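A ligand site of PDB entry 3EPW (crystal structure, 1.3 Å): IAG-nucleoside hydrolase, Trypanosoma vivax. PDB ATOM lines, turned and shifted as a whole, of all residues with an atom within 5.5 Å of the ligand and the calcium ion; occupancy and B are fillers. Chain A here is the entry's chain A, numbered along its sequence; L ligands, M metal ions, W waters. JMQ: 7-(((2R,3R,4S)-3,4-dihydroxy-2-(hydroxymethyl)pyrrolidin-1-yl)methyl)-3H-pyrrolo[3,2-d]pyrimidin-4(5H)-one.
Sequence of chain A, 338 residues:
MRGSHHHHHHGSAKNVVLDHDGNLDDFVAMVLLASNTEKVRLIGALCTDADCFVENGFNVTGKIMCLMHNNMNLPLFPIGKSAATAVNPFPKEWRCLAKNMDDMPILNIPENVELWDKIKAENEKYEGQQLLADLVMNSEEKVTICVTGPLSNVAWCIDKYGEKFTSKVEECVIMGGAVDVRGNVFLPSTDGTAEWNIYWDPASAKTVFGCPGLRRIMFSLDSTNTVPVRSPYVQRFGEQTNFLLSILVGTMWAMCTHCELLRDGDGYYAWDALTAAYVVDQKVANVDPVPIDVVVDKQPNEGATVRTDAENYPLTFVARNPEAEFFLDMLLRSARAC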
ATOM      1  N   ASP A  21      20.115  15.071 -22.728  1.00  0.00           N
ATOM      2  CA  ASP A  21      19.619  14.623 -24.026  1.00  0.00           C
ATOM      3  C   ASP A  21      18.293  15.220 -24.457  1.00  0.00           C
ATOM      4  O   ASP A  21      17.539  14.630 -25.225  1.00  0.00           O
ATOM      5  CB  ASP A  21      19.612  13.108 -24.137  1.00  0.00           C
ATOM      6  CG  ASP A  21      18.558  12.472 -23.273  1.00  0.00           C
ATOM      7  OD1 ASP A  21      18.105  13.115 -22.302  1.00  0.00           O
ATOM      8  OD2 ASP A  21      18.179  11.334 -23.589  1.00  0.00           O
ATOM      9  N   GLY A  22      18.029  16.426 -23.968  1.00  0.00           N
ATOM     10  CA  GLY A  22      17.071  17.295 -24.644  1.00  0.00           C
ATOM     11  C   GLY A  22      15.612  16.941 -24.539  1.00  0.00           C
ATOM     12  O   GLY A  22      14.826  17.401 -25.368  1.00  0.00           O
ATOM     13  N   ASN A  23      15.228  16.135 -23.555  1.00  0.00           N
ATOM     14  CA  ASN A  23      13.795  16.002 -23.284  1.00  0.00           C
ATOM     15  C   ASN A  23      13.321  17.084 -22.328  1.00  0.00           C
ATOM     16  O   ASN A  23      14.092  17.942 -21.920  1.00  0.00           O
ATOM     17  CB  ASN A  23      13.419  14.595 -22.815  1.00  0.00           C
ATOM     18  CG  ASN A  23      12.140  14.127 -23.448  1.00  0.00           C
ATOM     19  OD1 ASN A  23      11.066  14.209 -22.855  1.00  0.00           O
ATOM     20  ND2 ASN A  23      12.221  13.689 -24.699  1.00  0.00           N
ATOM     21  N   LEU A  24      12.039  17.071 -21.977  1.00  0.00           N
ATOM     22  CA  LEU A  24      11.478  18.169 -21.228  1.00  0.00           C
ATOM     23  C   LEU A  24      12.094  18.287 -19.859  1.00  0.00           C
ATOM     24  O   LEU A  24      12.463  19.386 -19.421  1.00  0.00           O
ATOM     25  CB  LEU A  24       9.973  18.014 -21.128  1.00  0.00           C
ATOM     26  CG  LEU A  24       9.234  18.029 -22.450  1.00  0.00           C
ATOM     27  CD1 LEU A  24       7.836  17.456 -22.210  1.00  0.00           C
ATOM     28  CD2 LEU A  24       9.170  19.422 -23.004  1.00  0.00           C
ATOM     29  N   ASP A  25      12.245  17.165 -19.157  1.00  0.00           N
ATOM     30  CA  ASP A  25      12.882  17.217 -17.860  1.00  0.00           C
ATOM     31  C   ASP A  25      14.354  17.596 -17.941  1.00  0.00           C
ATOM     32  O   ASP A  25      14.852  18.241 -17.031  1.00  0.00           O
ATOM     33  CB  ASP A  25      12.659  15.941 -17.051  1.00  0.00           C
ATOM     34  CG  ASP A  25      13.251  14.731 -17.697  1.00  0.00           C
ATOM     35  OD1 ASP A  25      13.458  14.744 -18.933  1.00  0.00           O
ATOM     36  OD2 ASP A  25      13.519  13.784 -16.919  1.00  0.00           O
ATOM     37  N   ASP A  26      15.051  17.259 -19.030  1.00  0.00           N
ATOM     38  CA  ASP A  26      16.419  17.736 -19.190  1.00  0.00           C
ATOM     39  C   ASP A  26      16.463  19.240 -19.123  1.00  0.00           C
ATOM     40  O   ASP A  26      17.354  19.808 -18.488  1.00  0.00           O
ATOM     41  CB  ASP A  26      17.014  17.306 -20.525  1.00  0.00           C
ATOM     42  CG  ASP A  26      17.147  15.812 -20.641  1.00  0.00           C
ATOM     43  OD1 ASP A  26      18.241  15.272 -20.342  1.00  0.00           O
ATOM     44  OD2 ASP A  26      16.142  15.161 -20.996  1.00  0.00           O
ATOM     45  N   ASP A  51      17.275  11.241 -26.430  1.00  0.00           N
ATOM     46  CA  ASP A  51      15.835  11.516 -26.306  1.00  0.00           C
ATOM     47  C   ASP A  51      15.444  12.865 -26.920  1.00  0.00           C
ATOM     48  O   ASP A  51      14.527  13.529 -26.461  1.00  0.00           O
ATOM     49  CB  ASP A  51      15.434  11.434 -24.845  1.00  0.00           C
ATOM     50  CG  ASP A  51      14.002  11.048 -24.648  1.00  0.00           C
ATOM     51  OD1 ASP A  51      13.306  10.648 -25.591  1.00  0.00           O
ATOM     52  OD2 ASP A  51      13.579  11.121 -23.456  1.00  0.00           O
ATOM     53  N   PHE A  90      15.910   5.935 -28.996  1.00  0.00           N
ATOM     54  CA  PHE A  90      14.630   6.280 -28.412  1.00  0.00           C
ATOM     55  C   PHE A  90      13.485   6.302 -29.422  1.00  0.00           C
ATOM     56  O   PHE A  90      13.723   6.499 -30.622  1.00  0.00           O
ATOM     57  CB  PHE A  90      14.727   7.667 -27.774  1.00  0.00           C
ATOM     58  CG  PHE A  90      15.255   7.649 -26.366  1.00  0.00           C
ATOM     59  CD1 PHE A  90      14.403   7.369 -25.315  1.00  0.00           C
ATOM     60  CD2 PHE A  90      16.567   7.963 -26.092  1.00  0.00           C
ATOM     61  CE1 PHE A  90      14.873   7.380 -24.020  1.00  0.00           C
ATOM     62  CE2 PHE A  90      17.033   7.969 -24.781  1.00  0.00           C
ATOM     63  CZ  PHE A  90      16.179   7.671 -23.743  1.00  0.00           C
ATOM     64  N   TRP A  94       9.050  10.513 -28.682  1.00  0.00           N
ATOM     65  CA  TRP A  94       9.637  11.134 -27.492  1.00  0.00           C
ATOM     66  C   TRP A  94      10.715  12.139 -27.881  1.00  0.00           C
ATOM     67  O   TRP A  94      10.890  13.150 -27.216  1.00  0.00           O
ATOM     68  CB  TRP A  94      10.250  10.094 -26.576  1.00  0.00           C
ATOM     69  CG  TRP A  94       9.301   9.120 -26.030  1.00  0.00           C
ATOM     70  CD1 TRP A  94       7.947   9.094 -26.179  1.00  0.00           C
ATOM     71  CD2 TRP A  94       9.628   8.007 -25.202  1.00  0.00           C
ATOM     72  NE1 TRP A  94       7.407   8.025 -25.509  1.00  0.00           N
ATOM     73  CE2 TRP A  94       8.432   7.343 -24.893  1.00  0.00           C
ATOM     74  CE3 TRP A  94      10.843   7.505 -24.702  1.00  0.00           C
ATOM     75  CZ2 TRP A  94       8.400   6.195 -24.116  1.00  0.00           C
ATOM     76  CZ3 TRP A  94      10.810   6.381 -23.905  1.00  0.00           C
ATOM     77  CH2 TRP A  94       9.604   5.738 -23.617  1.00  0.00           C
ATOM     78  N   LEU A  97      10.165  16.302 -28.645  1.00  0.00           N
ATOM     79  CA  LEU A  97       9.803  17.356 -27.706  1.00  0.00           C
ATOM     80  C   LEU A  97      10.693  18.587 -27.785  1.00  0.00           C
ATOM     81  O   LEU A  97      10.204  19.711 -27.608  1.00  0.00           O
ATOM     82  CB  LEU A  97       9.688  16.799 -26.287  1.00  0.00           C
ATOM     83  CG  LEU A  97       8.441  15.909 -26.108  1.00  0.00           C
ATOM     84  CD1 LEU A  97       8.518  15.017 -24.883  1.00  0.00           C
ATOM     85  CD2 LEU A  97       7.153  16.733 -26.093  1.00  0.00           C
ATOM     86  N   THR A 148      21.952  13.596 -17.482  1.00  0.00           N
ATOM     87  CA  THR A 148      20.514  13.385 -17.539  1.00  0.00           C
ATOM     88  C   THR A 148      20.079  12.676 -18.816  1.00  0.00           C
ATOM     89  O   THR A 148      18.897  12.421 -19.023  1.00  0.00           O
ATOM     90  CB  THR A 148      19.742  14.699 -17.340  1.00  0.00           C
ATOM     91  OG1 THR A 148      20.101  15.617 -18.370  1.00  0.00           O
ATOM     92  CG2 THR A 148      20.054  15.322 -15.999  1.00  0.00           C
ATOM     93  N   GLY A 149      21.058  12.374 -19.667  1.00  0.00           N
ATOM     94  CA  GLY A 149      20.837  11.464 -20.781  1.00  0.00           C
ATOM     95  C   GLY A 149      21.676  10.215 -20.578  1.00  0.00           C
ATOM     96  O   GLY A 149      22.100   9.927 -19.460  1.00  0.00           O
ATOM     97  N   MET A 175      21.038  10.506 -13.841  1.00  0.00           N
ATOM     98  CA  MET A 175      19.686   9.975 -13.914  1.00  0.00           C
ATOM     99  C   MET A 175      19.751   8.731 -14.770  1.00  0.00           C
ATOM    100  O   MET A 175      20.077   8.796 -15.950  1.00  0.00           O
ATOM    101  CB  MET A 175      18.708  10.974 -14.516  1.00  0.00           C
ATOM    102  CG  MET A 175      17.247  10.591 -14.321  1.00  0.00           C
ATOM    103  SD  MET A 175      16.714   9.264 -15.453  1.00  0.00           S
ATOM    104  CE  MET A 175      16.061   8.040 -14.337  1.00  0.00           C
ATOM    105  N   ASN A 184      11.664   0.967 -17.374  1.00  0.00           N
ATOM    106  CA  ASN A 184      10.668   1.639 -18.186  1.00  0.00           C
ATOM    107  C   ASN A 184      10.820   1.382 -19.679  1.00  0.00           C
ATOM    108  O   ASN A 184      10.179   2.045 -20.486  1.00  0.00           O
ATOM    109  CB  ASN A 184      10.588   3.144 -17.858  1.00  0.00           C
ATOM    110  CG  ASN A 184      11.866   3.908 -18.151  1.00  0.00           C
ATOM    111  OD1 ASN A 184      12.783   3.420 -18.835  1.00  0.00           O
ATOM    112  ND2 ASN A 184      11.924   5.133 -17.650  1.00  0.00           N
ATOM    113  N   GLU A 195      15.978   0.658 -17.632  1.00  0.00           N
ATOM    114  CA  GLU A 195      15.594   2.036 -17.784  1.00  0.00           C
ATOM    115  C   GLU A 195      16.246   2.613 -19.044  1.00  0.00           C
ATOM    116  O   GLU A 195      17.337   2.208 -19.448  1.00  0.00           O
ATOM    117  CB  GLU A 195      15.991   2.788 -16.516  1.00  0.00           C
ATOM    118  CG  GLU A 195      15.672   4.284 -16.525  1.00  0.00           C
ATOM    119  CD  GLU A 195      16.695   5.097 -17.315  1.00  0.00           C
ATOM    120  OE1 GLU A 195      17.890   4.707 -17.329  1.00  0.00           O
ATOM    121  OE2 GLU A 195      16.313   6.134 -17.913  1.00  0.00           O
ATOM    122  N   TRP A 196      15.547   3.555 -19.671  1.00  0.00           N
ATOM    123  CA  TRP A 196      15.890   4.012 -21.003  1.00  0.00           C
ATOM    124  C   TRP A 196      17.257   4.645 -21.182  1.00  0.00           C
ATOM    125  O   TRP A 196      17.920   4.369 -22.174  1.00  0.00           O
ATOM    126  CB  TRP A 196      14.799   4.968 -21.531  1.00  0.00           C
ATOM    127  CG  TRP A 196      13.833   4.268 -22.423  1.00  0.00           C
ATOM    128  CD1 TRP A 196      12.551   3.864 -22.129  1.00  0.00           C
ATOM    129  CD2 TRP A 196      14.079   3.870 -23.767  1.00  0.00           C
ATOM    130  NE1 TRP A 196      12.000   3.222 -23.210  1.00  0.00           N
ATOM    131  CE2 TRP A 196      12.905   3.223 -24.229  1.00  0.00           C
ATOM    132  CE3 TRP A 196      15.170   3.994 -24.628  1.00  0.00           C
ATOM    133  CZ2 TRP A 196      12.816   2.700 -25.528  1.00  0.00           C
ATOM    134  CZ3 TRP A 196      15.084   3.471 -25.913  1.00  0.00           C
ATOM    135  CH2 TRP A 196      13.908   2.838 -26.346  1.00  0.00           C
ATOM    136  N   ASN A 197      17.691   5.499 -20.266  1.00  0.00           N
ATOM    137  CA  ASN A 197      18.992   6.123 -20.422  1.00  0.00           C
ATOM    138  C   ASN A 197      20.106   5.102 -20.490  1.00  0.00           C
ATOM    139  O   ASN A 197      21.089   5.272 -21.228  1.00  0.00           O
ATOM    140  CB  ASN A 197      19.262   7.106 -19.296  1.00  0.00           C
ATOM    141  CG  ASN A 197      18.500   8.403 -19.469  1.00  0.00           C
ATOM    142  OD1 ASN A 197      17.869   8.618 -20.498  1.00  0.00           O
ATOM    143  ND2 ASN A 197      18.538   9.259 -18.447  1.00  0.00           N
ATOM    144  N   LEU A 221      15.079   4.792 -11.090  1.00  0.00           N
ATOM    145  CA  LEU A 221      13.640   4.902 -11.018  1.00  0.00           C
ATOM    146  C   LEU A 221      13.152   4.701  -9.600  1.00  0.00           C
ATOM    147  O   LEU A 221      12.100   5.205  -9.235  1.00  0.00           O
ATOM    148  CB  LEU A 221      12.967   3.924 -11.964  1.00  0.00           C
ATOM    149  CG  LEU A 221      13.333   4.124 -13.441  1.00  0.00           C
ATOM    150  CD1 LEU A 221      12.502   3.193 -14.295  1.00  0.00           C
ATOM    151  CD2 LEU A 221      13.112   5.578 -13.862  1.00  0.00           C
ATOM    152  N   CYS A 259       0.841  11.774 -20.166  1.00  0.00           N
ATOM    153  CA  CYS A 259       1.529  10.522 -20.474  1.00  0.00           C
ATOM    154  C   CYS A 259       0.948   9.364 -19.693  1.00  0.00           C
ATOM    155  O   CYS A 259       0.897   8.244 -20.197  1.00  0.00           O
ATOM    156  CB  CYS A 259       3.025  10.641 -20.213  1.00  0.00           C
ATOM    157  SG  CYS A 259       3.866  11.818 -21.274  1.00  0.00           S
ATOM    158  N   ARG A 263      -0.224   5.654 -20.815  1.00  0.00           N
ATOM    159  CA  ARG A 263       0.403   4.477 -20.226  1.00  0.00           C
ATOM    160  C   ARG A 263       0.051   4.434 -18.764  1.00  0.00           C
ATOM    161  O   ARG A 263       0.707   5.067 -17.933  1.00  0.00           O
ATOM    162  CB  ARG A 263       1.918   4.560 -20.359  1.00  0.00           C
ATOM    163  CG  ARG A 263       2.463   4.517 -21.771  1.00  0.00           C
ATOM    164  CD  ARG A 263       3.993   4.396 -21.746  1.00  0.00           C
ATOM    165  NE  ARG A 263       4.567   5.361 -20.813  1.00  0.00           N
ATOM    166  CZ  ARG A 263       5.201   6.480 -21.167  1.00  0.00           C
ATOM    167  NH1 ARG A 263       5.411   6.763 -22.447  1.00  0.00           N
ATOM    168  NH2 ARG A 263       5.646   7.296 -20.228  1.00  0.00           N
ATOM    169  N   GLY A 267       3.492   7.108 -16.421  1.00  0.00           N
ATOM    170  CA  GLY A 267       3.549   8.396 -17.127  1.00  0.00           C
ATOM    171  C   GLY A 267       4.921   9.016 -17.146  1.00  0.00           C
ATOM    172  O   GLY A 267       5.956   8.332 -17.128  1.00  0.00           O
ATOM    173  N   TYR A 268       4.925  10.336 -17.186  1.00  0.00           N
ATOM    174  CA  TYR A 268       6.148  11.115 -17.176  1.00  0.00           C
ATOM    175  C   TYR A 268       6.493  11.473 -15.741  1.00  0.00           C
ATOM    176  O   TYR A 268       5.597  11.710 -14.925  1.00  0.00           O
ATOM    177  CB  TYR A 268       5.941  12.387 -18.008  1.00  0.00           C
ATOM    178  CG  TYR A 268       7.192  12.983 -18.631  1.00  0.00           C
ATOM    179  CD1 TYR A 268       7.522  12.732 -19.955  1.00  0.00           C
ATOM    180  CD2 TYR A 268       7.998  13.836 -17.896  1.00  0.00           C
ATOM    181  CE1 TYR A 268       8.649  13.305 -20.525  1.00  0.00           C
ATOM    182  CE2 TYR A 268       9.122  14.415 -18.458  1.00  0.00           C
ATOM    183  CZ  TYR A 268       9.427  14.151 -19.768  1.00  0.00           C
ATOM    184  OH  TYR A 268      10.566  14.722 -20.304  1.00  0.00           O
ATOM    185  N   TRP A 271      12.185  13.092 -13.765  1.00  0.00           N
ATOM    186  CA  TRP A 271      13.377  12.261 -13.582  1.00  0.00           C
ATOM    187  C   TRP A 271      14.650  13.114 -13.466  1.00  0.00           C
ATOM    188  O   TRP A 271      15.409  13.016 -12.484  1.00  0.00           O
ATOM    189  CB  TRP A 271      13.566  11.342 -14.776  1.00  0.00           C
ATOM    190  CG  TRP A 271      12.494  10.309 -15.115  1.00  0.00           C
ATOM    191  CD1 TRP A 271      12.322   9.073 -14.561  1.00  0.00           C
ATOM    192  CD2 TRP A 271      11.568  10.370 -16.222  1.00  0.00           C
ATOM    193  NE1 TRP A 271      11.333   8.393 -15.209  1.00  0.00           N
ATOM    194  CE2 TRP A 271      10.861   9.158 -16.238  1.00  0.00           C
ATOM    195  CE3 TRP A 271      11.261  11.349 -17.175  1.00  0.00           C
ATOM    196  CZ2 TRP A 271       9.877   8.884 -17.174  1.00  0.00           C
ATOM    197  CZ3 TRP A 271      10.270  11.069 -18.109  1.00  0.00           C
ATOM    198  CH2 TRP A 271       9.601   9.849 -18.104  1.00  0.00           C
ATOM    199  N   ASP A 272      14.887  13.943 -14.483  1.00  0.00           N
ATOM    200  CA  ASP A 272      16.141  14.659 -14.584  1.00  0.00           C
ATOM    201  C   ASP A 272      16.129  15.859 -13.672  1.00  0.00           C
ATOM    202  O   ASP A 272      17.191  16.300 -13.219  1.00  0.00           O
ATOM    203  CB  ASP A 272      16.364  15.131 -16.013  1.00  0.00           C
ATOM    204  CG  ASP A 272      16.526  14.003 -16.981  1.00  0.00           C
ATOM    205  OD1 ASP A 272      16.665  12.845 -16.549  1.00  0.00           O
ATOM    206  OD2 ASP A 272      16.550  14.287 -18.210  1.00  0.00           O
HETATM  207  C1  JMQ L   1      13.592   8.656 -21.268  1.00  0.00           C
HETATM  208  C2  JMQ L   1      10.094  10.892 -23.108  1.00  0.00           C
HETATM  209  C8  JMQ L   1      11.399   7.518 -20.529  1.00  0.00           C
HETATM  210  C9  JMQ L   1      12.060   8.475 -21.195  1.00  0.00           C
HETATM  211  O6  JMQ L   1       7.556   8.884 -21.695  1.00  0.00           O
HETATM  212  C6  JMQ L   1       8.698   9.303 -21.972  1.00  0.00           C
HETATM  213  N1  JMQ L   1       8.826  10.404 -22.781  1.00  0.00           N
HETATM  214  N3  JMQ L   1      11.176  10.315 -22.637  1.00  0.00           N
HETATM  215  C4  JMQ L   1      11.089   9.247 -21.825  1.00  0.00           C
HETATM  216  C5  JMQ L   1       9.851   8.709 -21.487  1.00  0.00           C
HETATM  217  N7  JMQ L   1      10.081   7.667 -20.700  1.00  0.00           N
HETATM  218  N4' JMQ L   1      14.137   9.780 -20.435  1.00  0.00           N
HETATM  219  C1' JMQ L   1      13.196  10.885 -20.130  1.00  0.00           C
HETATM  220  C2' JMQ L   1      13.976  11.756 -19.165  1.00  0.00           C
HETATM  221  O2' JMQ L   1      14.664  12.779 -19.916  1.00  0.00           O
HETATM  222  C3' JMQ L   1      14.950  10.805 -18.442  1.00  0.00           C
HETATM  223  O3' JMQ L   1      16.315  11.238 -18.554  1.00  0.00           O
HETATM  224  C4' JMQ L   1      14.775   9.433 -19.122  1.00  0.00           C
HETATM  225  C5' JMQ L   1      13.943   8.489 -18.234  1.00  0.00           C
HETATM  226  O5' JMQ L   1      14.020   7.117 -18.645  1.00  0.00           O
HETATM  227 CA    CA M   1      16.996  13.010 -20.200  1.00  0.00          CA
HETATM  228  O   HOH W   1       6.906  12.008 -23.933  1.00  0.00           O
HETATM  229  O   HOH W   2      16.633  10.810 -21.390  1.00  0.00           O
HETATM  230  O   HOH W   3       8.495   5.760 -19.604  1.00  0.00           O
HETATM  231  O   HOH W   4       4.862   9.641 -23.641  1.00  0.00           O
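The backbone carbonyl oxygen (O) of Gly 267 is in hydrogen-bond range of the guanidinium group (NH2) of Arg 263.
The side-chain hydroxyl (OH) of Tyr 268 lies within hydrogen-bond range of the backbone NH (N) of Leu 24.
The side-chain carboxylate (OD2) of Asp 26 sits close to the backbone NH (N) of Asn 23.
The backbone NH (N) of Asp 51 is in hydrogen-bond range of the side-chain carboxylate (OD2) of Asp 21, 3.0 Å away.
The side-chain carboxylate (OD2) of Asp 25 sits close to the backbone NH (N) of Trp 271.
N of Asp 25 lies within hydrogen-bond range of OH of Tyr 268, 3.2 Å away.
The backbone carbonyl oxygen of Asp 51 lies within hydrogen-bond range of the side-chain amide nitrogen of Asn 23.
OD1 of Asn 184 is in hydrogen-bond range of N of Trp 196 (2.9 Å).
Water W2 lies within hydrogen-bond range of the side-chain amide oxygen (OD1) of Asn 197 and the side-chain carboxylate (OD2) of Asp 21.
Water W3 lies within hydrogen-bond range of a nitrogen (N7) of the ligand (2.7 Å) and the guanidinium group (NH2) of Arg 263 (3.3 Å).
Water W4 lies within hydrogen-bond range of NH1 of Arg 263 (3.2 Å), SG of Cys 259 (3.4 Å) and O6 of the ligand (3.4 Å).
OD1 of Asn 23 touches C2 of the ligand, 3.5 Å away.
CE1 of Phe 90 touches C1 of the ligand, 3.3 Å away.
CE3 of Trp 94 touches C4 of the ligand, 3.4 Å away.
Trp 196 touches the ligand (CB to O5', 3.7 Å).
Tyr 268 touches the ligand (CE1 to N1, 3.7 Å).
Trp 271 touches the ligand.
Of the 24 residues printed, 16 come within 4 Å of the ligand.
Of the 24 residues printed, 4 come within 4 Å of the calcium ion.
The nearest printed residue that does not touch the calcium ion is Asp 25 (4.1 Å).
The backbone carbonyl oxygen (O) of Thr 148 is bound to the calcium ion, 2.3 Å away.
The calcium ion is bound by an oxygen (O2') of the ligand (2.4 Å).
The side-chain carboxylate (OD1) of Asp 21 is bound to the calcium ion (2.4 Å).
OD2 of Asp 272 binds the calcium ion (2.4 Å).
The calcium ion is bound by OD2 of Asp 26 (2.4 Å).
O3' of the ligand binds the calcium ion, at 2.5 Å.
Water W2 is bound to the calcium ion.
The calcium ion is bound by the side-chain carboxylate (OD1) of Asp 26 (2.6 Å).
The calcium ion has eight donor atoms within binding distance.
The side-chain carboxylate (OD1) of Asp 25 sits close to an oxygen (O2') of the ligand, 2.5 Å away.
The side-chain carboxylate of Asp 51 lies within salt-bridge range of a nitrogen (N4') of the ligand.
The side-chain amide nitrogen of Asn 197 lies close to an oxygen (O3') of the ligand.
The side-chain amide nitrogen (ND2) of Asn 184 lies within hydrogen-bond range of an oxygen (O5') of the ligand (3.1 Å).
The side-chain carboxylate of Glu 195 is in hydrogen-bond range of an oxygen (O5') of the ligand (2.6 Å).
NH2 of Arg 263 sits at hydrogen-bond distance from O6 of the ligand (2.9 Å).
The side-chain sulfur (SD) of Met 175 lies close to an oxygen (O3') of the ligand (3.7 Å).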
